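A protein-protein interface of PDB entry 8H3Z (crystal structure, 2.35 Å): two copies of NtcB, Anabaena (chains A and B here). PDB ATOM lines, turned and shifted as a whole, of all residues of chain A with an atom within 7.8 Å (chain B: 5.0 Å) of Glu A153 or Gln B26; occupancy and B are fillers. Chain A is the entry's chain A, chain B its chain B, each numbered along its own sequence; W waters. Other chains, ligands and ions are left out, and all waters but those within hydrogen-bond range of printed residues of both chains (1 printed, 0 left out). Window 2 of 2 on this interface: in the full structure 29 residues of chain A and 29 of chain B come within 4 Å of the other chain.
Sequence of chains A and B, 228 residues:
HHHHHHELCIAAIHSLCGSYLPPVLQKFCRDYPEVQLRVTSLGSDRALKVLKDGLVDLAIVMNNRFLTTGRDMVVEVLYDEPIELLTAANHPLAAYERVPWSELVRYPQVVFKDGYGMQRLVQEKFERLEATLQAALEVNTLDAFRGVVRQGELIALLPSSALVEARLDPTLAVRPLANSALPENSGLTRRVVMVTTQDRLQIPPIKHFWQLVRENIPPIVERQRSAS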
ATOM      1  N   ALA A  88     -22.565 -18.897 -13.771  1.00  0.00           N
ATOM      2  CA  ALA A  88     -23.075 -20.072 -14.464  1.00  0.00           C
ATOM      3  C   ALA A  88     -24.251 -19.657 -15.339  1.00  0.00           C
ATOM      4  O   ALA A  88     -25.042 -18.789 -14.957  1.00  0.00           O
ATOM      5  CB  ALA A  88     -23.525 -21.148 -13.496  1.00  0.00           C
ATOM      6  N   HIS A  91     -27.490 -19.521 -13.648  1.00  0.00           N
ATOM      7  CA  HIS A  91     -27.568 -18.717 -12.443  1.00  0.00           C
ATOM      8  C   HIS A  91     -28.747 -17.760 -12.553  1.00  0.00           C
ATOM      9  O   HIS A  91     -28.955 -17.163 -13.611  1.00  0.00           O
ATOM     10  CB  HIS A  91     -26.252 -17.967 -12.197  1.00  0.00           C
ATOM     11  CG  HIS A  91     -26.189 -17.420 -10.814  1.00  0.00           C
ATOM     12  ND1 HIS A  91     -26.713 -16.202 -10.441  1.00  0.00           N
ATOM     13  CD2 HIS A  91     -25.667 -17.960  -9.709  1.00  0.00           C
ATOM     14  CE1 HIS A  91     -26.507 -16.042  -9.140  1.00  0.00           C
ATOM     15  NE2 HIS A  91     -25.895 -17.103  -8.680  1.00  0.00           N
ATOM     16  N   PRO A  92     -29.535 -17.558 -11.472  1.00  0.00           N
ATOM     17  CA  PRO A  92     -30.664 -16.624 -11.497  1.00  0.00           C
ATOM     18  C   PRO A  92     -30.349 -15.260 -12.104  1.00  0.00           C
ATOM     19  O   PRO A  92     -31.184 -14.704 -12.818  1.00  0.00           O
ATOM     20  CB  PRO A  92     -31.019 -16.456 -10.007  1.00  0.00           C
ATOM     21  CG  PRO A  92     -30.618 -17.774  -9.379  1.00  0.00           C
ATOM     22  CD  PRO A  92     -29.399 -18.224 -10.170  1.00  0.00           C
ATOM     23  N   TYR A 107     -25.350 -12.367  -3.368  1.00  0.00           N
ATOM     24  CA  TYR A 107     -24.828 -13.668  -3.753  1.00  0.00           C
ATOM     25  C   TYR A 107     -23.358 -13.812  -3.371  1.00  0.00           C
ATOM     26  O   TYR A 107     -22.547 -12.901  -3.533  1.00  0.00           O
ATOM     27  CB  TYR A 107     -25.041 -13.928  -5.247  1.00  0.00           C
ATOM     28  CG  TYR A 107     -26.486 -14.137  -5.622  1.00  0.00           C
ATOM     29  CD1 TYR A 107     -27.303 -13.053  -5.902  1.00  0.00           C
ATOM     30  CD2 TYR A 107     -27.050 -15.409  -5.664  1.00  0.00           C
ATOM     31  CE1 TYR A 107     -28.633 -13.227  -6.247  1.00  0.00           C
ATOM     32  CE2 TYR A 107     -28.391 -15.596  -5.983  1.00  0.00           C
ATOM     33  CZ  TYR A 107     -29.183 -14.499  -6.283  1.00  0.00           C
ATOM     34  OH  TYR A 107     -30.509 -14.636  -6.630  1.00  0.00           O
ATOM     35  N   PRO A 108     -22.977 -14.981  -2.823  1.00  0.00           N
ATOM     36  CA  PRO A 108     -21.577 -15.249  -2.494  1.00  0.00           C
ATOM     37  C   PRO A 108     -20.683 -15.295  -3.730  1.00  0.00           C
ATOM     38  O   PRO A 108     -21.083 -15.815  -4.776  1.00  0.00           O
ATOM     39  CB  PRO A 108     -21.644 -16.611  -1.789  1.00  0.00           C
ATOM     40  CG  PRO A 108     -22.922 -17.234  -2.289  1.00  0.00           C
ATOM     41  CD  PRO A 108     -23.881 -16.081  -2.432  1.00  0.00           C
ATOM     42  N   GLN A 109     -19.458 -14.772  -3.586  1.00  0.00           N
ATOM     43  CA  GLN A 109     -18.590 -14.542  -4.732  1.00  0.00           C
ATOM     44  C   GLN A 109     -17.294 -15.330  -4.638  1.00  0.00           C
ATOM     45  O   GLN A 109     -16.834 -15.614  -3.541  1.00  0.00           O
ATOM     46  CB  GLN A 109     -18.206 -13.069  -4.816  1.00  0.00           C
ATOM     47  CG  GLN A 109     -19.359 -12.161  -5.202  1.00  0.00           C
ATOM     48  CD  GLN A 109     -18.804 -10.817  -5.570  1.00  0.00           C
ATOM     49  OE1 GLN A 109     -17.609 -10.674  -5.852  1.00  0.00           O
ATOM     50  NE2 GLN A 109     -19.669  -9.819  -5.539  1.00  0.00           N
ATOM     51  N   VAL A 110     -16.722 -15.651  -5.810  1.00  0.00           N
ATOM     52  CA  VAL A 110     -15.295 -15.919  -5.940  1.00  0.00           C
ATOM     53  C   VAL A 110     -14.613 -14.582  -6.148  1.00  0.00           C
ATOM     54  O   VAL A 110     -15.090 -13.765  -6.943  1.00  0.00           O
ATOM     55  CB  VAL A 110     -14.868 -16.782  -7.146  1.00  0.00           C
ATOM     56  CG1 VAL A 110     -13.358 -16.881  -7.228  1.00  0.00           C
ATOM     57  CG2 VAL A 110     -15.503 -18.143  -7.196  1.00  0.00           C
ATOM     58  N   ALA A 136     -16.458 -16.164  -0.392  1.00  0.00           N
ATOM     59  CA  ALA A 136     -16.346 -17.580  -0.080  1.00  0.00           C
ATOM     60  C   ALA A 136     -15.022 -18.183  -0.575  1.00  0.00           C
ATOM     61  O   ALA A 136     -14.522 -19.135   0.004  1.00  0.00           O
ATOM     62  CB  ALA A 136     -17.534 -18.302  -0.667  1.00  0.00           C
ATOM     63  N   LEU A 137     -14.452 -17.671  -1.668  1.00  0.00           N
ATOM     64  CA  LEU A 137     -13.292 -18.324  -2.249  1.00  0.00           C
ATOM     65  C   LEU A 137     -12.359 -17.286  -2.848  1.00  0.00           C
ATOM     66  O   LEU A 137     -12.805 -16.350  -3.512  1.00  0.00           O
ATOM     67  CB  LEU A 137     -13.787 -19.346  -3.282  1.00  0.00           C
ATOM     68  CG  LEU A 137     -12.738 -20.027  -4.164  1.00  0.00           C
ATOM     69  CD1 LEU A 137     -11.760 -20.882  -3.363  1.00  0.00           C
ATOM     70  CD2 LEU A 137     -13.436 -20.883  -5.204  1.00  0.00           C
ATOM     71  N   VAL A 148     -14.638 -22.749 -11.237  1.00  0.00           N
ATOM     72  CA  VAL A 148     -15.421 -22.653 -10.022  1.00  0.00           C
ATOM     73  C   VAL A 148     -16.831 -22.128 -10.326  1.00  0.00           C
ATOM     74  O   VAL A 148     -17.809 -22.666  -9.805  1.00  0.00           O
ATOM     75  CB  VAL A 148     -14.619 -21.783  -9.030  1.00  0.00           C
ATOM     76  CG1 VAL A 148     -15.448 -21.183  -7.921  1.00  0.00           C
ATOM     77  CG2 VAL A 148     -13.446 -22.566  -8.455  1.00  0.00           C
ATOM     78  N   VAL A 149     -16.938 -21.073 -11.156  1.00  0.00           N
ATOM     79  CA  VAL A 149     -18.226 -20.469 -11.480  1.00  0.00           C
ATOM     80  C   VAL A 149     -19.136 -21.423 -12.275  1.00  0.00           C
ATOM     81  O   VAL A 149     -20.358 -21.348 -12.143  1.00  0.00           O
ATOM     82  CB  VAL A 149     -18.049 -19.128 -12.214  1.00  0.00           C
ATOM     83  CG1 VAL A 149     -19.360 -18.627 -12.777  1.00  0.00           C
ATOM     84  CG2 VAL A 149     -17.427 -18.073 -11.312  1.00  0.00           C
ATOM     85  N   ARG A 150     -18.562 -22.392 -12.994  1.00  0.00           N
ATOM     86  CA  ARG A 150     -19.402 -23.392 -13.718  1.00  0.00           C
ATOM     87  C   ARG A 150     -20.171 -24.275 -12.724  1.00  0.00           C
ATOM     88  O   ARG A 150     -21.034 -25.046 -13.183  1.00  0.00           O
ATOM     89  CB  ARG A 150     -18.529 -24.252 -14.634  1.00  0.00           C
ATOM     90  CG  ARG A 150     -18.291 -23.643 -16.008  1.00  0.00           C
ATOM     91  CD  ARG A 150     -16.896 -23.958 -16.506  1.00  0.00           C
ATOM     92  NE  ARG A 150     -16.436 -23.005 -17.502  1.00  0.00           N
ATOM     93  CZ  ARG A 150     -15.160 -22.755 -17.765  1.00  0.00           C
ATOM     94  NH1 ARG A 150     -14.211 -23.391 -17.100  1.00  0.00           N
ATOM     95  NH2 ARG A 150     -14.838 -21.873 -18.693  1.00  0.00           N
ATOM     96  N   GLN A 151     -19.877 -24.172 -11.426  1.00  0.00           N
ATOM     97  CA  GLN A 151     -20.513 -24.973 -10.379  1.00  0.00           C
ATOM     98  C   GLN A 151     -21.784 -24.327  -9.811  1.00  0.00           C
ATOM     99  O   GLN A 151     -22.496 -24.965  -9.032  1.00  0.00           O
ATOM    100  CB  GLN A 151     -19.564 -25.170  -9.190  1.00  0.00           C
ATOM    101  CG  GLN A 151     -18.264 -25.919  -9.494  1.00  0.00           C
ATOM    102  CD  GLN A 151     -18.415 -27.420  -9.442  1.00  0.00           C
ATOM    103  OE1 GLN A 151     -18.925 -27.975  -8.472  1.00  0.00           O
ATOM    104  NE2 GLN A 151     -17.964 -28.095 -10.486  1.00  0.00           N
ATOM    105  N   GLY A 152     -22.071 -23.064 -10.150  1.00  0.00           N
ATOM    106  CA  GLY A 152     -23.410 -22.505  -9.975  1.00  0.00           C
ATOM    107  C   GLY A 152     -23.718 -21.971  -8.570  1.00  0.00           C
ATOM    108  O   GLY A 152     -24.852 -21.606  -8.282  1.00  0.00           O
ATOM    109  N   GLU A 153     -22.726 -21.926  -7.683  1.00  0.00           N
ATOM    110  CA  GLU A 153     -22.890 -21.319  -6.372  1.00  0.00           C
ATOM    111  C   GLU A 153     -22.394 -19.876  -6.420  1.00  0.00           C
ATOM    112  O   GLU A 153     -23.013 -18.989  -5.841  1.00  0.00           O
ATOM    113  CB  GLU A 153     -22.112 -22.106  -5.303  1.00  0.00           C
ATOM    114  CG  GLU A 153     -22.596 -23.529  -5.046  1.00  0.00           C
ATOM    115  CD  GLU A 153     -24.043 -23.706  -4.616  1.00  0.00           C
ATOM    116  OE1 GLU A 153     -24.531 -22.887  -3.807  1.00  0.00           O
ATOM    117  OE2 GLU A 153     -24.688 -24.656  -5.112  1.00  0.00           O
ATOM    118  N   LEU A 154     -21.263 -19.649  -7.099  1.00  0.00           N
ATOM    119  CA  LEU A 154     -20.501 -18.426  -6.905  1.00  0.00           C
ATOM    120  C   LEU A 154     -20.553 -17.611  -8.199  1.00  0.00           C
ATOM    121  O   LEU A 154     -20.790 -18.147  -9.281  1.00  0.00           O
ATOM    122  CB  LEU A 154     -19.063 -18.791  -6.490  1.00  0.00           C
ATOM    123  CG  LEU A 154     -18.816 -19.502  -5.142  1.00  0.00           C
ATOM    124  CD1 LEU A 154     -17.394 -19.931  -4.914  1.00  0.00           C
ATOM    125  CD2 LEU A 154     -19.226 -18.626  -3.967  1.00  0.00           C
ATOM    126  N   ILE A 155     -20.385 -16.302  -8.047  1.00  0.00           N
ATOM    127  CA  ILE A 155     -20.390 -15.332  -9.137  1.00  0.00           C
ATOM    128  C   ILE A 155     -19.114 -14.506  -8.989  1.00  0.00           C
ATOM    129  O   ILE A 155     -18.518 -14.504  -7.922  1.00  0.00           O
ATOM    130  CB  ILE A 155     -21.669 -14.471  -9.059  1.00  0.00           C
ATOM    131  CG1 ILE A 155     -21.616 -13.442  -7.924  1.00  0.00           C
ATOM    132  CG2 ILE A 155     -22.895 -15.367  -8.912  1.00  0.00           C
ATOM    133  CD1 ILE A 155     -22.770 -12.463  -7.916  1.00  0.00           C
ATOM    134  N   PRO B  22     -12.981 -28.180  -8.498  1.00  0.00           N
ATOM    135  CA  PRO B  22     -14.196 -27.453  -8.099  1.00  0.00           C
ATOM    136  C   PRO B  22     -15.267 -28.266  -7.366  1.00  0.00           C
ATOM    137  O   PRO B  22     -15.813 -27.784  -6.371  1.00  0.00           O
ATOM    138  CB  PRO B  22     -14.714 -26.908  -9.439  1.00  0.00           C
ATOM    139  CG  PRO B  22     -13.455 -26.726 -10.268  1.00  0.00           C
ATOM    140  CD  PRO B  22     -12.607 -27.918  -9.902  1.00  0.00           C
ATOM    141  N   PRO B  23     -15.604 -29.507  -7.809  1.00  0.00           N
ATOM    142  CA  PRO B  23     -16.454 -30.405  -7.025  1.00  0.00           C
ATOM    143  C   PRO B  23     -16.067 -30.569  -5.553  1.00  0.00           C
ATOM    144  O   PRO B  23     -16.960 -30.579  -4.696  1.00  0.00           O
ATOM    145  CB  PRO B  23     -16.305 -31.755  -7.756  1.00  0.00           C
ATOM    146  CG  PRO B  23     -16.072 -31.371  -9.199  1.00  0.00           C
ATOM    147  CD  PRO B  23     -15.243 -30.106  -9.111  1.00  0.00           C
ATOM    148  N   VAL B  24     -14.750 -30.663  -5.273  1.00  0.00           N
ATOM    149  CA  VAL B  24     -14.229 -30.816  -3.914  1.00  0.00           C
ATOM    150  C   VAL B  24     -14.420 -29.524  -3.115  1.00  0.00           C
ATOM    151  O   VAL B  24     -14.784 -29.563  -1.931  1.00  0.00           O
ATOM    152  CB  VAL B  24     -12.735 -31.177  -3.918  1.00  0.00           C
ATOM    153  CG1 VAL B  24     -12.196 -31.326  -2.505  1.00  0.00           C
ATOM    154  CG2 VAL B  24     -12.449 -32.406  -4.752  1.00  0.00           C
ATOM    155  N   LEU B  25     -14.176 -28.382  -3.772  1.00  0.00           N
ATOM    156  CA  LEU B  25     -14.297 -27.080  -3.123  1.00  0.00           C
ATOM    157  C   LEU B  25     -15.722 -26.877  -2.618  1.00  0.00           C
ATOM    158  O   LEU B  25     -15.915 -26.411  -1.495  1.00  0.00           O
ATOM    159  CB  LEU B  25     -13.940 -25.947  -4.099  1.00  0.00           C
ATOM    160  CG  LEU B  25     -12.553 -26.000  -4.735  1.00  0.00           C
ATOM    161  CD1 LEU B  25     -12.223 -24.682  -5.398  1.00  0.00           C
ATOM    162  CD2 LEU B  25     -11.499 -26.341  -3.714  1.00  0.00           C
ATOM    163  N   GLN B  26     -16.695 -27.177  -3.502  1.00  0.00           N
ATOM    164  CA  GLN B  26     -18.118 -27.072  -3.205  1.00  0.00           C
ATOM    165  C   GLN B  26     -18.506 -28.024  -2.059  1.00  0.00           C
ATOM    166  O   GLN B  26     -19.165 -27.596  -1.119  1.00  0.00           O
ATOM    167  CB  GLN B  26     -18.931 -27.349  -4.476  1.00  0.00           C
ATOM    168  CG  GLN B  26     -20.426 -27.091  -4.331  1.00  0.00           C
ATOM    169  CD  GLN B  26     -21.219 -27.499  -5.554  1.00  0.00           C
ATOM    170  OE1 GLN B  26     -20.750 -28.248  -6.403  1.00  0.00           O
ATOM    171  NE2 GLN B  26     -22.443 -27.009  -5.656  1.00  0.00           N
ATOM    172  N   LYS B  27     -18.132 -29.312  -2.124  1.00  0.00           N
ATOM    173  CA  LYS B  27     -18.467 -30.241  -1.046  1.00  0.00           C
ATOM    174  C   LYS B  27     -17.910 -29.716   0.284  1.00  0.00           C
ATOM    175  O   LYS B  27     -18.621 -29.690   1.289  1.00  0.00           O
ATOM    176  CB  LYS B  27     -17.937 -31.664  -1.276  1.00  0.00           C
ATOM    177  CG  LYS B  27     -18.514 -32.446  -2.456  1.00  0.00           C
ATOM    178  CD  LYS B  27     -18.063 -33.906  -2.467  1.00  0.00           C
ATOM    179  CE  LYS B  27     -18.012 -34.540  -3.845  1.00  0.00           C
ATOM    180  NZ  LYS B  27     -16.755 -34.234  -4.566  1.00  0.00           N
ATOM    181  N   PHE B  28     -16.647 -29.266   0.287  1.00  0.00           N
ATOM    182  CA  PHE B  28     -16.037 -28.759   1.505  1.00  0.00           C
ATOM    183  C   PHE B  28     -16.837 -27.588   2.094  1.00  0.00           C
ATOM    184  O   PHE B  28     -17.128 -27.593   3.291  1.00  0.00           O
ATOM    185  CB  PHE B  28     -14.572 -28.385   1.281  1.00  0.00           C
ATOM    186  CG  PHE B  28     -13.928 -27.811   2.515  1.00  0.00           C
ATOM    187  CD1 PHE B  28     -14.021 -26.456   2.799  1.00  0.00           C
ATOM    188  CD2 PHE B  28     -13.266 -28.627   3.415  1.00  0.00           C
ATOM    189  CE1 PHE B  28     -13.445 -25.925   3.946  1.00  0.00           C
ATOM    190  CE2 PHE B  28     -12.702 -28.099   4.565  1.00  0.00           C
ATOM    191  CZ  PHE B  28     -12.790 -26.753   4.828  1.00  0.00           C
ATOM    192  N   CYS B  29     -17.210 -26.600   1.275  1.00  0.00           N
ATOM    193  CA  CYS B  29     -17.927 -25.422   1.758  1.00  0.00           C
ATOM    194  C   CYS B  29     -19.297 -25.788   2.329  1.00  0.00           C
ATOM    195  O   CYS B  29     -19.712 -25.226   3.343  1.00  0.00           O
ATOM    196  CB  CYS B  29     -18.109 -24.364   0.678  1.00  0.00           C
ATOM    197  SG  CYS B  29     -16.544 -23.681   0.081  1.00  0.00           S
ATOM    198  N   ARG B  30     -19.988 -26.732   1.676  1.00  0.00           N
ATOM    199  CA  ARG B  30     -21.230 -27.296   2.176  1.00  0.00           C
ATOM    200  C   ARG B  30     -21.023 -27.801   3.605  1.00  0.00           C
ATOM    201  O   ARG B  30     -21.848 -27.534   4.480  1.00  0.00           O
ATOM    202  CB  ARG B  30     -21.676 -28.393   1.203  1.00  0.00           C
ATOM    203  CG  ARG B  30     -22.869 -29.244   1.630  1.00  0.00           C
ATOM    204  CD  ARG B  30     -22.747 -30.617   0.989  1.00  0.00           C
ATOM    205  NE  ARG B  30     -23.958 -31.423   0.962  1.00  0.00           N
ATOM    206  CZ  ARG B  30     -24.377 -32.215   1.946  1.00  0.00           C
ATOM    207  NH1 ARG B  30     -23.716 -32.260   3.088  1.00  0.00           N
ATOM    208  NH2 ARG B  30     -25.461 -32.958   1.782  1.00  0.00           N
HETATM  209  O   HOH W   1     -23.131 -27.906  -8.958  1.00  0.00           O
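Of chain B, only Gln B26 (3.3 Å) comes within 4 Å of Glu A153. Gln B26 touches just these residues of chain A: Gln A151 and Glu A153. Printed residues of chain A within 4 Å of Leu B25: Leu A137 (3.99 Å) and Val A148 (3.9 Å). Of the printed residues of chain A, Pro B23 touches Gln A151. Of the printed residues of chain A, Pro B22 touches Gln A151 (3.6 Å). Of the printed residues of chain B, Gln A151 touches Pro B22 (3.6 Å), Pro B23 (3.7 Å) and Gln B26 (2.8 Å). Arg B30 touches none of the printed residues of chain A. The nearest residue of chain A that does not touch Gln B26 is Gly A152 (6.0 Å). The nearest printed residue of chain A that does not touch Pro B23 is Val A148 (7.2 Å).
No position is printed for both chains. Of the 6 pairs that touch across the chains among the printed residues, none has its exchanged pair printed and touching as well.
Among the printed residues, pairs that only touch across the chains: Leu A137 with Leu B25, Val A148 with Leu B25, Gln A151 with Pro B22 and Gln A151 with Pro B23.
Of the 17 printed residues of chain A, 4 touch a printed residue of chain B. Of the 9 printed residues of chain B, 4 touch a printed residue of chain A. Hydrophobic or aromatic side chains of chain B within 4 Å of the printed part of chain A: Pro B22, Pro B23 and Leu B25. Among the printed residues, 6 pairs touch across the chains.
Water W1 lies within hydrogen-bond range of the backbone carbonyl oxygen (O) of Gln A151 (3.0 Å) and the side-chain amide nitrogen (NE2) of Gln B26 (3.5 Å).
OE1 of Gln A151 sits close to OE1 of Gln B26 (2.8 Å). The side-chain carboxylate (OE2) of Glu A153 sits at hydrogen-bond distance from the side-chain amide nitrogen (NE2) of Gln B26, 3.3 Å away.
O of Leu B25 is in hydrogen-bond range of SG of Cys B29 (3.2 Å).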
